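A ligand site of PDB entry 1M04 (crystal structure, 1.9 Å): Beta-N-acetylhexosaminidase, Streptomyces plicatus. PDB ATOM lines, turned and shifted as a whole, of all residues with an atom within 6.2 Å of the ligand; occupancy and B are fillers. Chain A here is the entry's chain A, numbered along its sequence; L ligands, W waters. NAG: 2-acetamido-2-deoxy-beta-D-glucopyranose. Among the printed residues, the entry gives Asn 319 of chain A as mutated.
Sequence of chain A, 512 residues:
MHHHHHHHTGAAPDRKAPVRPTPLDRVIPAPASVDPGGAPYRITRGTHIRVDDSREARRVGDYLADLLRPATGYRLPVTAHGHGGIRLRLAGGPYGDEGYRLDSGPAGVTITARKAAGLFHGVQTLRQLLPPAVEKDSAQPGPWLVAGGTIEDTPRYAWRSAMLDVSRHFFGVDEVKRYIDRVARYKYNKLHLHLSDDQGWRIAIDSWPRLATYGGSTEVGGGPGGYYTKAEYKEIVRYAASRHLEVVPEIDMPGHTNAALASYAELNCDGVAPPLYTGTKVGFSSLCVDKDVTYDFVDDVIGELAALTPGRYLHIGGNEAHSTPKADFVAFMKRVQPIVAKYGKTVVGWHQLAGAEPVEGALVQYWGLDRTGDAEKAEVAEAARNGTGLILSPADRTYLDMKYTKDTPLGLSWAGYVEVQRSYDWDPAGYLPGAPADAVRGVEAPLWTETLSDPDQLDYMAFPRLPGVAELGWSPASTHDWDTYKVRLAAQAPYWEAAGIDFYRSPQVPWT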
ATOM      1  N   ASP A 165       1.486 -26.865   1.322  1.00  0.00           N
ATOM      2  CA  ASP A 165       1.092 -25.726   2.151  1.00  0.00           C
ATOM      3  C   ASP A 165       1.100 -26.205   3.597  1.00  0.00           C
ATOM      4  O   ASP A 165       0.250 -26.989   4.008  1.00  0.00           O
ATOM      5  CB  ASP A 165      -0.316 -25.269   1.719  1.00  0.00           C
ATOM      6  CG  ASP A 165      -0.963 -24.302   2.705  1.00  0.00           C
ATOM      7  OD1 ASP A 165      -0.316 -23.866   3.679  1.00  0.00           O
ATOM      8  OD2 ASP A 165      -2.157 -23.989   2.476  1.00  0.00           O
ATOM      9  N   ARG A 168      -1.655 -23.408   6.387  1.00  0.00           N
ATOM     10  CA  ARG A 168      -3.079 -23.533   6.702  1.00  0.00           C
ATOM     11  C   ARG A 168      -3.254 -24.608   7.770  1.00  0.00           C
ATOM     12  O   ARG A 168      -3.969 -24.401   8.751  1.00  0.00           O
ATOM     13  CB  ARG A 168      -3.873 -23.852   5.428  1.00  0.00           C
ATOM     14  CG  ARG A 168      -4.261 -22.600   4.631  1.00  0.00           C
ATOM     15  CD  ARG A 168      -3.106 -21.598   4.507  1.00  0.00           C
ATOM     16  NE  ARG A 168      -3.529 -20.378   3.813  1.00  0.00           N
ATOM     17  CZ  ARG A 168      -3.684 -20.283   2.498  1.00  0.00           C
ATOM     18  NH1 ARG A 168      -3.451 -21.340   1.720  1.00  0.00           N
ATOM     19  NH2 ARG A 168      -4.118 -19.154   1.955  1.00  0.00           N
ATOM     20  N   HIS A 194       5.332 -23.794   1.317  1.00  0.00           N
ATOM     21  CA  HIS A 194       4.618 -22.540   1.608  1.00  0.00           C
ATOM     22  C   HIS A 194       4.707 -22.409   3.122  1.00  0.00           C
ATOM     23  O   HIS A 194       3.832 -22.879   3.855  1.00  0.00           O
ATOM     24  CB  HIS A 194       3.158 -22.681   1.164  1.00  0.00           C
ATOM     25  CG  HIS A 194       2.410 -21.380   1.112  1.00  0.00           C
ATOM     26  ND1 HIS A 194       2.629 -20.437   0.140  1.00  0.00           N
ATOM     27  CD2 HIS A 194       1.434 -20.881   1.914  1.00  0.00           C
ATOM     28  CE1 HIS A 194       1.827 -19.403   0.338  1.00  0.00           C
ATOM     29  NE2 HIS A 194       1.087 -19.643   1.410  1.00  0.00           N
ATOM     30  N   ASP A 197       1.641 -17.836   5.968  1.00  0.00           N
ATOM     31  CA  ASP A 197       0.412 -17.332   5.396  1.00  0.00           C
ATOM     32  C   ASP A 197      -0.364 -16.641   6.509  1.00  0.00           C
ATOM     33  O   ASP A 197       0.210 -16.246   7.526  1.00  0.00           O
ATOM     34  CB  ASP A 197      -0.398 -18.472   4.777  1.00  0.00           C
ATOM     35  CG  ASP A 197      -1.255 -17.999   3.620  1.00  0.00           C
ATOM     36  OD1 ASP A 197      -2.268 -17.304   3.863  1.00  0.00           O
ATOM     37  OD2 ASP A 197      -0.903 -18.305   2.455  1.00  0.00           O
ATOM     38  N   ASP A 252       5.457 -15.656   1.874  1.00  0.00           N
ATOM     39  CA  ASP A 252       4.542 -14.834   1.094  1.00  0.00           C
ATOM     40  C   ASP A 252       4.480 -13.375   1.521  1.00  0.00           C
ATOM     41  O   ASP A 252       4.297 -13.071   2.709  1.00  0.00           O
ATOM     42  CB  ASP A 252       3.136 -15.430   1.142  1.00  0.00           C
ATOM     43  CG  ASP A 252       2.317 -15.163  -0.108  1.00  0.00           C
ATOM     44  OD1 ASP A 252       2.616 -14.162  -0.818  1.00  0.00           O
ATOM     45  OD2 ASP A 252       1.377 -15.942  -0.386  1.00  0.00           O
ATOM     46  N   HIS A 256      -1.098 -12.171   2.438  1.00  0.00           N
ATOM     47  CA  HIS A 256      -1.002 -13.441   3.158  1.00  0.00           C
ATOM     48  C   HIS A 256       0.036 -13.349   4.283  1.00  0.00           C
ATOM     49  O   HIS A 256       0.813 -14.281   4.525  1.00  0.00           O
ATOM     50  CB  HIS A 256      -0.635 -14.561   2.187  1.00  0.00           C
ATOM     51  CG  HIS A 256      -1.764 -14.975   1.297  1.00  0.00           C
ATOM     52  ND1 HIS A 256      -2.761 -15.830   1.711  1.00  0.00           N
ATOM     53  CD2 HIS A 256      -2.085 -14.611   0.034  1.00  0.00           C
ATOM     54  CE1 HIS A 256      -3.648 -15.977   0.738  1.00  0.00           C
ATOM     55  NE2 HIS A 256      -3.259 -15.243  -0.297  1.00  0.00           N
ATOM     56  N   VAL A 282      -9.061 -15.417   1.981  1.00  0.00           N
ATOM     57  CA  VAL A 282      -7.788 -14.831   1.545  1.00  0.00           C
ATOM     58  C   VAL A 282      -7.953 -13.389   1.080  1.00  0.00           C
ATOM     59  O   VAL A 282      -9.076 -12.914   0.870  1.00  0.00           O
ATOM     60  CB  VAL A 282      -7.183 -15.617   0.362  1.00  0.00           C
ATOM     61  CG1 VAL A 282      -7.067 -17.103   0.712  1.00  0.00           C
ATOM     62  CG2 VAL A 282      -8.047 -15.433  -0.890  1.00  0.00           C
ATOM     63  N   ASN A 319       1.015 -13.145  -4.247  1.00  0.00           N
ATOM     64  CA  ASN A 319      -0.359 -13.416  -4.677  1.00  0.00           C
ATOM     65  C   ASN A 319      -1.416 -12.841  -3.738  1.00  0.00           C
ATOM     66  O   ASN A 319      -1.175 -12.650  -2.549  1.00  0.00           O
ATOM     67  CB  ASN A 319      -0.593 -14.919  -4.736  1.00  0.00           C
ATOM     68  CG  ASN A 319      -0.455 -15.561  -3.372  1.00  0.00           C
ATOM     69  OD1 ASN A 319       0.584 -15.458  -2.735  1.00  0.00           O
ATOM     70  ND2 ASN A 319      -1.516 -16.220  -2.909  1.00  0.00           N
ATOM     71  N   GLU A 320      -2.584 -12.586  -4.303  1.00  0.00           N
ATOM     72  CA  GLU A 320      -3.734 -12.109  -3.566  1.00  0.00           C
ATOM     73  C   GLU A 320      -3.479 -11.013  -2.534  1.00  0.00           C
ATOM     74  O   GLU A 320      -3.985 -11.061  -1.418  1.00  0.00           O
ATOM     75  CB  GLU A 320      -4.416 -13.321  -2.900  1.00  0.00           C
ATOM     76  CG  GLU A 320      -4.698 -14.438  -3.907  1.00  0.00           C
ATOM     77  CD  GLU A 320      -5.217 -15.720  -3.271  1.00  0.00           C
ATOM     78  OE1 GLU A 320      -4.697 -16.143  -2.217  1.00  0.00           O
ATOM     79  OE2 GLU A 320      -6.146 -16.324  -3.854  1.00  0.00           O
ATOM     80  N   TRP A 350       4.595 -15.481  -7.521  1.00  0.00           N
ATOM     81  CA  TRP A 350       3.407 -15.913  -8.254  1.00  0.00           C
ATOM     82  C   TRP A 350       3.288 -14.931  -9.417  1.00  0.00           C
ATOM     83  O   TRP A 350       3.910 -13.874  -9.365  1.00  0.00           O
ATOM     84  CB  TRP A 350       2.174 -15.901  -7.338  1.00  0.00           C
ATOM     85  CG  TRP A 350       2.282 -16.897  -6.223  1.00  0.00           C
ATOM     86  CD1 TRP A 350       2.608 -16.648  -4.917  1.00  0.00           C
ATOM     87  CD2 TRP A 350       2.101 -18.324  -6.320  1.00  0.00           C
ATOM     88  NE1 TRP A 350       2.638 -17.821  -4.193  1.00  0.00           N
ATOM     89  CE2 TRP A 350       2.326 -18.859  -5.029  1.00  0.00           C
ATOM     90  CE3 TRP A 350       1.764 -19.187  -7.366  1.00  0.00           C
ATOM     91  CZ2 TRP A 350       2.230 -20.227  -4.761  1.00  0.00           C
ATOM     92  CZ3 TRP A 350       1.659 -20.554  -7.103  1.00  0.00           C
ATOM     93  CH2 TRP A 350       1.895 -21.059  -5.802  1.00  0.00           C
ATOM     94  N   GLN A 352       1.533 -12.553 -10.260  1.00  0.00           N
ATOM     95  CA  GLN A 352       1.143 -11.160 -10.030  1.00  0.00           C
ATOM     96  C   GLN A 352       2.422 -10.325 -10.113  1.00  0.00           C
ATOM     97  O   GLN A 352       2.377  -9.124 -10.398  1.00  0.00           O
ATOM     98  CB  GLN A 352       0.490 -10.989  -8.649  1.00  0.00           C
ATOM     99  CG  GLN A 352      -0.984 -11.414  -8.593  1.00  0.00           C
ATOM    100  CD  GLN A 352      -1.187 -12.888  -8.860  1.00  0.00           C
ATOM    101  OE1 GLN A 352      -0.498 -13.728  -8.286  1.00  0.00           O
ATOM    102  NE2 GLN A 352      -2.141 -13.214  -9.733  1.00  0.00           N
ATOM    103  N   TRP A 367      -0.631 -19.251 -11.985  1.00  0.00           N
ATOM    104  CA  TRP A 367      -1.693 -20.085 -11.438  1.00  0.00           C
ATOM    105  C   TRP A 367      -3.061 -19.741 -12.051  1.00  0.00           C
ATOM    106  O   TRP A 367      -4.104 -20.082 -11.483  1.00  0.00           O
ATOM    107  CB  TRP A 367      -1.739 -19.964  -9.906  1.00  0.00           C
ATOM    108  CG  TRP A 367      -1.886 -18.555  -9.372  1.00  0.00           C
ATOM    109  CD1 TRP A 367      -0.909 -17.591  -9.289  1.00  0.00           C
ATOM    110  CD2 TRP A 367      -3.062 -17.972  -8.819  1.00  0.00           C
ATOM    111  NE1 TRP A 367      -1.411 -16.451  -8.714  1.00  0.00           N
ATOM    112  CE2 TRP A 367      -2.733 -16.653  -8.423  1.00  0.00           C
ATOM    113  CE3 TRP A 367      -4.371 -18.434  -8.609  1.00  0.00           C
ATOM    114  CZ2 TRP A 367      -3.669 -15.787  -7.833  1.00  0.00           C
ATOM    115  CZ3 TRP A 367      -5.304 -17.570  -8.028  1.00  0.00           C
ATOM    116  CH2 TRP A 367      -4.946 -16.270  -7.649  1.00  0.00           C
ATOM    117  N   ALA A 395      -4.640 -23.178 -11.693  1.00  0.00           N
ATOM    118  CA  ALA A 395      -5.547 -23.533 -10.595  1.00  0.00           C
ATOM    119  C   ALA A 395      -6.590 -24.558 -11.034  1.00  0.00           C
ATOM    120  O   ALA A 395      -7.095 -25.324 -10.205  1.00  0.00           O
ATOM    121  CB  ALA A 395      -6.252 -22.273 -10.076  1.00  0.00           C
ATOM    122  N   TYR A 399      -3.833 -27.821  -9.266  1.00  0.00           N
ATOM    123  CA  TYR A 399      -4.068 -27.539  -7.849  1.00  0.00           C
ATOM    124  C   TYR A 399      -4.659 -28.834  -7.277  1.00  0.00           C
ATOM    125  O   TYR A 399      -5.788 -29.196  -7.593  1.00  0.00           O
ATOM    126  CB  TYR A 399      -5.066 -26.394  -7.679  1.00  0.00           C
ATOM    127  CG  TYR A 399      -4.450 -25.023  -7.521  1.00  0.00           C
ATOM    128  CD1 TYR A 399      -3.216 -24.706  -8.117  1.00  0.00           C
ATOM    129  CD2 TYR A 399      -5.123 -24.016  -6.827  1.00  0.00           C
ATOM    130  CE1 TYR A 399      -2.676 -23.418  -8.010  1.00  0.00           C
ATOM    131  CE2 TYR A 399      -4.593 -22.726  -6.725  1.00  0.00           C
ATOM    132  CZ  TYR A 399      -3.374 -22.437  -7.322  1.00  0.00           C
ATOM    133  OH  TYR A 399      -2.852 -21.165  -7.209  1.00  0.00           O
ATOM    134  N   ASP A 401      -5.687 -29.431  -4.385  1.00  0.00           N
ATOM    135  CA  ASP A 401      -6.729 -29.211  -3.380  1.00  0.00           C
ATOM    136  C   ASP A 401      -8.094 -29.020  -4.047  1.00  0.00           C
ATOM    137  O   ASP A 401      -9.107 -28.929  -3.361  1.00  0.00           O
ATOM    138  CB  ASP A 401      -6.405 -27.987  -2.514  1.00  0.00           C
ATOM    139  CG  ASP A 401      -6.404 -26.695  -3.306  1.00  0.00           C
ATOM    140  OD1 ASP A 401      -5.817 -26.673  -4.412  1.00  0.00           O
ATOM    141  OD2 ASP A 401      -6.962 -25.687  -2.818  1.00  0.00           O
ATOM    142  N   MET A 402      -8.120 -28.945  -5.376  1.00  0.00           N
ATOM    143  CA  MET A 402      -9.398 -28.735  -6.073  1.00  0.00           C
ATOM    144  C   MET A 402     -10.177 -30.051  -6.162  1.00  0.00           C
ATOM    145  O   MET A 402      -9.608 -31.107  -6.442  1.00  0.00           O
ATOM    146  CB  MET A 402      -9.165 -28.158  -7.473  1.00  0.00           C
ATOM    147  CG  MET A 402     -10.210 -27.142  -7.917  1.00  0.00           C
ATOM    148  SD  MET A 402     -10.339 -25.705  -6.805  1.00  0.00           S
ATOM    149  CE  MET A 402      -8.640 -25.105  -6.806  1.00  0.00           C
ATOM    150  N   LEU A 412     -11.492 -27.705  -2.419  1.00  0.00           N
ATOM    151  CA  LEU A 412     -12.255 -26.524  -2.790  1.00  0.00           C
ATOM    152  C   LEU A 412     -12.800 -26.627  -4.222  1.00  0.00           C
ATOM    153  O   LEU A 412     -12.449 -27.540  -4.965  1.00  0.00           O
ATOM    154  CB  LEU A 412     -11.378 -25.284  -2.649  1.00  0.00           C
ATOM    155  CG  LEU A 412     -10.843 -25.015  -1.237  1.00  0.00           C
ATOM    156  CD1 LEU A 412     -10.044 -23.712  -1.214  1.00  0.00           C
ATOM    157  CD2 LEU A 412     -12.009 -24.926  -0.250  1.00  0.00           C
ATOM    158  N   TRP A 414     -13.631 -23.371  -6.151  1.00  0.00           N
ATOM    159  CA  TRP A 414     -13.699 -22.053  -6.779  1.00  0.00           C
ATOM    160  C   TRP A 414     -13.143 -22.035  -8.203  1.00  0.00           C
ATOM    161  O   TRP A 414     -13.555 -21.213  -9.016  1.00  0.00           O
ATOM    162  CB  TRP A 414     -12.964 -21.024  -5.933  1.00  0.00           C
ATOM    163  CG  TRP A 414     -11.489 -21.248  -5.828  1.00  0.00           C
ATOM    164  CD1 TRP A 414     -10.838 -21.981  -4.878  1.00  0.00           C
ATOM    165  CD2 TRP A 414     -10.487 -20.743  -6.713  1.00  0.00           C
ATOM    166  NE1 TRP A 414      -9.477 -21.957  -5.122  1.00  0.00           N
ATOM    167  CE2 TRP A 414      -9.235 -21.203  -6.241  1.00  0.00           C
ATOM    168  CE3 TRP A 414     -10.525 -19.953  -7.872  1.00  0.00           C
ATOM    169  CZ2 TRP A 414      -8.034 -20.895  -6.885  1.00  0.00           C
ATOM    170  CZ3 TRP A 414      -9.326 -19.634  -8.508  1.00  0.00           C
ATOM    171  CH2 TRP A 414      -8.093 -20.117  -8.006  1.00  0.00           C
ATOM    172  N   TRP A 448      -2.695 -27.079  -1.521  1.00  0.00           N
ATOM    173  CA  TRP A 448      -3.096 -26.119  -0.485  1.00  0.00           C
ATOM    174  C   TRP A 448      -3.828 -26.893   0.611  1.00  0.00           C
ATOM    175  O   TRP A 448      -4.504 -27.886   0.327  1.00  0.00           O
ATOM    176  CB  TRP A 448      -4.010 -25.047  -1.083  1.00  0.00           C
ATOM    177  CG  TRP A 448      -3.340 -24.306  -2.224  1.00  0.00           C
ATOM    178  CD1 TRP A 448      -3.518 -24.508  -3.561  1.00  0.00           C
ATOM    179  CD2 TRP A 448      -2.323 -23.304  -2.097  1.00  0.00           C
ATOM    180  NE1 TRP A 448      -2.686 -23.687  -4.282  1.00  0.00           N
ATOM    181  CE2 TRP A 448      -1.938 -22.935  -3.412  1.00  0.00           C
ATOM    182  CE3 TRP A 448      -1.702 -22.673  -1.011  1.00  0.00           C
ATOM    183  CZ2 TRP A 448      -0.951 -21.975  -3.662  1.00  0.00           C
ATOM    184  CZ3 TRP A 448      -0.724 -21.711  -1.265  1.00  0.00           C
ATOM    185  CH2 TRP A 448      -0.363 -21.369  -2.585  1.00  0.00           C
ATOM    186  N   THR A 449      -3.723 -26.439   1.856  1.00  0.00           N
ATOM    187  CA  THR A 449      -4.325 -27.202   2.944  1.00  0.00           C
ATOM    188  C   THR A 449      -5.442 -26.613   3.806  1.00  0.00           C
ATOM    189  O   THR A 449      -5.557 -26.967   4.973  1.00  0.00           O
ATOM    190  CB  THR A 449      -3.219 -27.758   3.876  1.00  0.00           C
ATOM    191  OG1 THR A 449      -2.432 -26.667   4.394  1.00  0.00           O
ATOM    192  CG2 THR A 449      -2.299 -28.706   3.094  1.00  0.00           C
ATOM    193  N   GLU A 450      -6.268 -25.731   3.247  1.00  0.00           N
ATOM    194  CA  GLU A 450      -7.365 -25.177   4.036  1.00  0.00           C
ATOM    195  C   GLU A 450      -8.269 -26.295   4.565  1.00  0.00           C
ATOM    196  O   GLU A 450      -8.796 -26.206   5.674  1.00  0.00           O
ATOM    197  CB  GLU A 450      -8.235 -24.227   3.204  1.00  0.00           C
ATOM    198  CG  GLU A 450      -7.673 -22.823   3.035  1.00  0.00           C
ATOM    199  CD  GLU A 450      -6.877 -22.663   1.759  1.00  0.00           C
ATOM    200  OE1 GLU A 450      -6.292 -23.653   1.291  1.00  0.00           O
ATOM    201  OE2 GLU A 450      -6.839 -21.532   1.224  1.00  0.00           O
HETATM  202  C1  NAG L   1      -4.670 -20.280  -4.476  1.00  0.00           C
HETATM  203  C2  NAG L   1      -4.069 -19.275  -3.484  1.00  0.00           C
HETATM  204  C3  NAG L   1      -4.070 -19.814  -2.039  1.00  0.00           C
HETATM  205  C4  NAG L   1      -5.323 -20.604  -1.638  1.00  0.00           C
HETATM  206  C5  NAG L   1      -5.775 -21.517  -2.783  1.00  0.00           C
HETATM  207  C6  NAG L   1      -7.069 -22.245  -2.528  1.00  0.00           C
HETATM  208  C7  NAG L   1      -2.446 -18.132  -4.865  1.00  0.00           C
HETATM  209  C8  NAG L   1      -1.111 -18.285  -5.577  1.00  0.00           C
HETATM  210  N2  NAG L   1      -2.704 -18.982  -3.877  1.00  0.00           N
HETATM  211  O1  NAG L   1      -4.872 -19.680  -5.703  1.00  0.00           O
HETATM  212  O3  NAG L   1      -3.855 -18.736  -1.134  1.00  0.00           O
HETATM  213  O4  NAG L   1      -5.037 -21.389  -0.498  1.00  0.00           O
HETATM  214  O5  NAG L   1      -5.928 -20.750  -3.991  1.00  0.00           O
HETATM  215  O6  NAG L   1      -7.354 -23.162  -3.582  1.00  0.00           O
HETATM  216  O7  NAG L   1      -3.226 -17.242  -5.200  1.00  0.00           O
HETATM  217  O   HOH W   1      -7.849 -18.301  -3.258  1.00  0.00           O
HETATM  218  O   HOH W   2      -1.190 -17.970  -0.445  1.00  0.00           O
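The side-chain carboxylate of Glu 450 is in hydrogen-bond range of an oxygen (O4) of the ligand (2.5 Å).
O6 of the ligand lies within hydrogen-bond range of OD2 of Asp 401.
The guanidinium group of Arg 168 sits at hydrogen-bond distance from an oxygen (O4) of the ligand (2.7 Å).
NE1 of Trp 414 is in hydrogen-bond range of O6 of the ligand, at 2.9 Å.
The side-chain amide nitrogen of Asn 319 lies close to an oxygen (O7) of the ligand, at 3.0 Å.
An oxygen (O1) of the ligand is in hydrogen-bond range of the side-chain hydroxyl (OH) of Tyr 399, at 2.9 Å.
The side-chain carboxylate (OE1) of Glu 320 is in hydrogen-bond range of an oxygen (O3) of the ligand, at 2.9 Å.
Merely in contact with the ligand: Trp 367 (3.0 Å), Trp 350 (3.3 Å), His 256 (3.3 Å), Trp 448 (3.5 Å), Leu 412 (3.6 Å) and Met 402 (3.98 Å).
Hydrophobic or aromatic side chains within 4 Å of the ligand: His 256, Trp 350, Trp 367, Tyr 399, Met 402, Leu 412, Trp 414 and Trp 448.
The nearest printed residue that does not touch the ligand is Val 282 (4.05 Å).
OE2 of Glu 450 lies within salt-bridge range of NH1 of Arg 168 (3.4 Å).
The backbone NH (N) of Leu 412 lies within hydrogen-bond range of the backbone carbonyl oxygen (O) of Asp 401 (2.8 Å).
The guanidinium group (NH2) of Arg 168 is in salt-bridge range of the side-chain carboxylate (OD1) of Asp 197, at 3.2 Å.
OE1 of Glu 320 sits at hydrogen-bond distance from ND2 of Asn 319.
OD1 of Asn 319 sits close to NE1 of Trp 350 (3.5 Å).
The side-chain amide oxygen (OD1) of Asn 319 sits close to the side-chain carboxylate (OD2) of Asp 252, at 2.5 Å.
OE1 of Glu 320 is in hydrogen-bond range of NE2 of His 256.
OD1 of Asp 197 lies within hydrogen-bond range of ND1 of His 256.
Water W2 lies within hydrogen-bond range of an oxygen (O3) of the ligand (2.9 Å), the side-chain carboxylate (OD2) of Asp 197 (2.9 Å), the side-chain amide nitrogen (ND2) of Asn 319 (3.0 Å), the side-chain carboxylate (OD2) of Asp 252 (3.3 Å), a ring nitrogen (NE2) of His 194 (3.4 Å) and a ring nitrogen (ND1) of His 256 (3.4 Å).
Water W1 lies within hydrogen-bond range of OE2 of Glu 320 (2.7 Å) and O5 of the ligand (3.2 Å).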
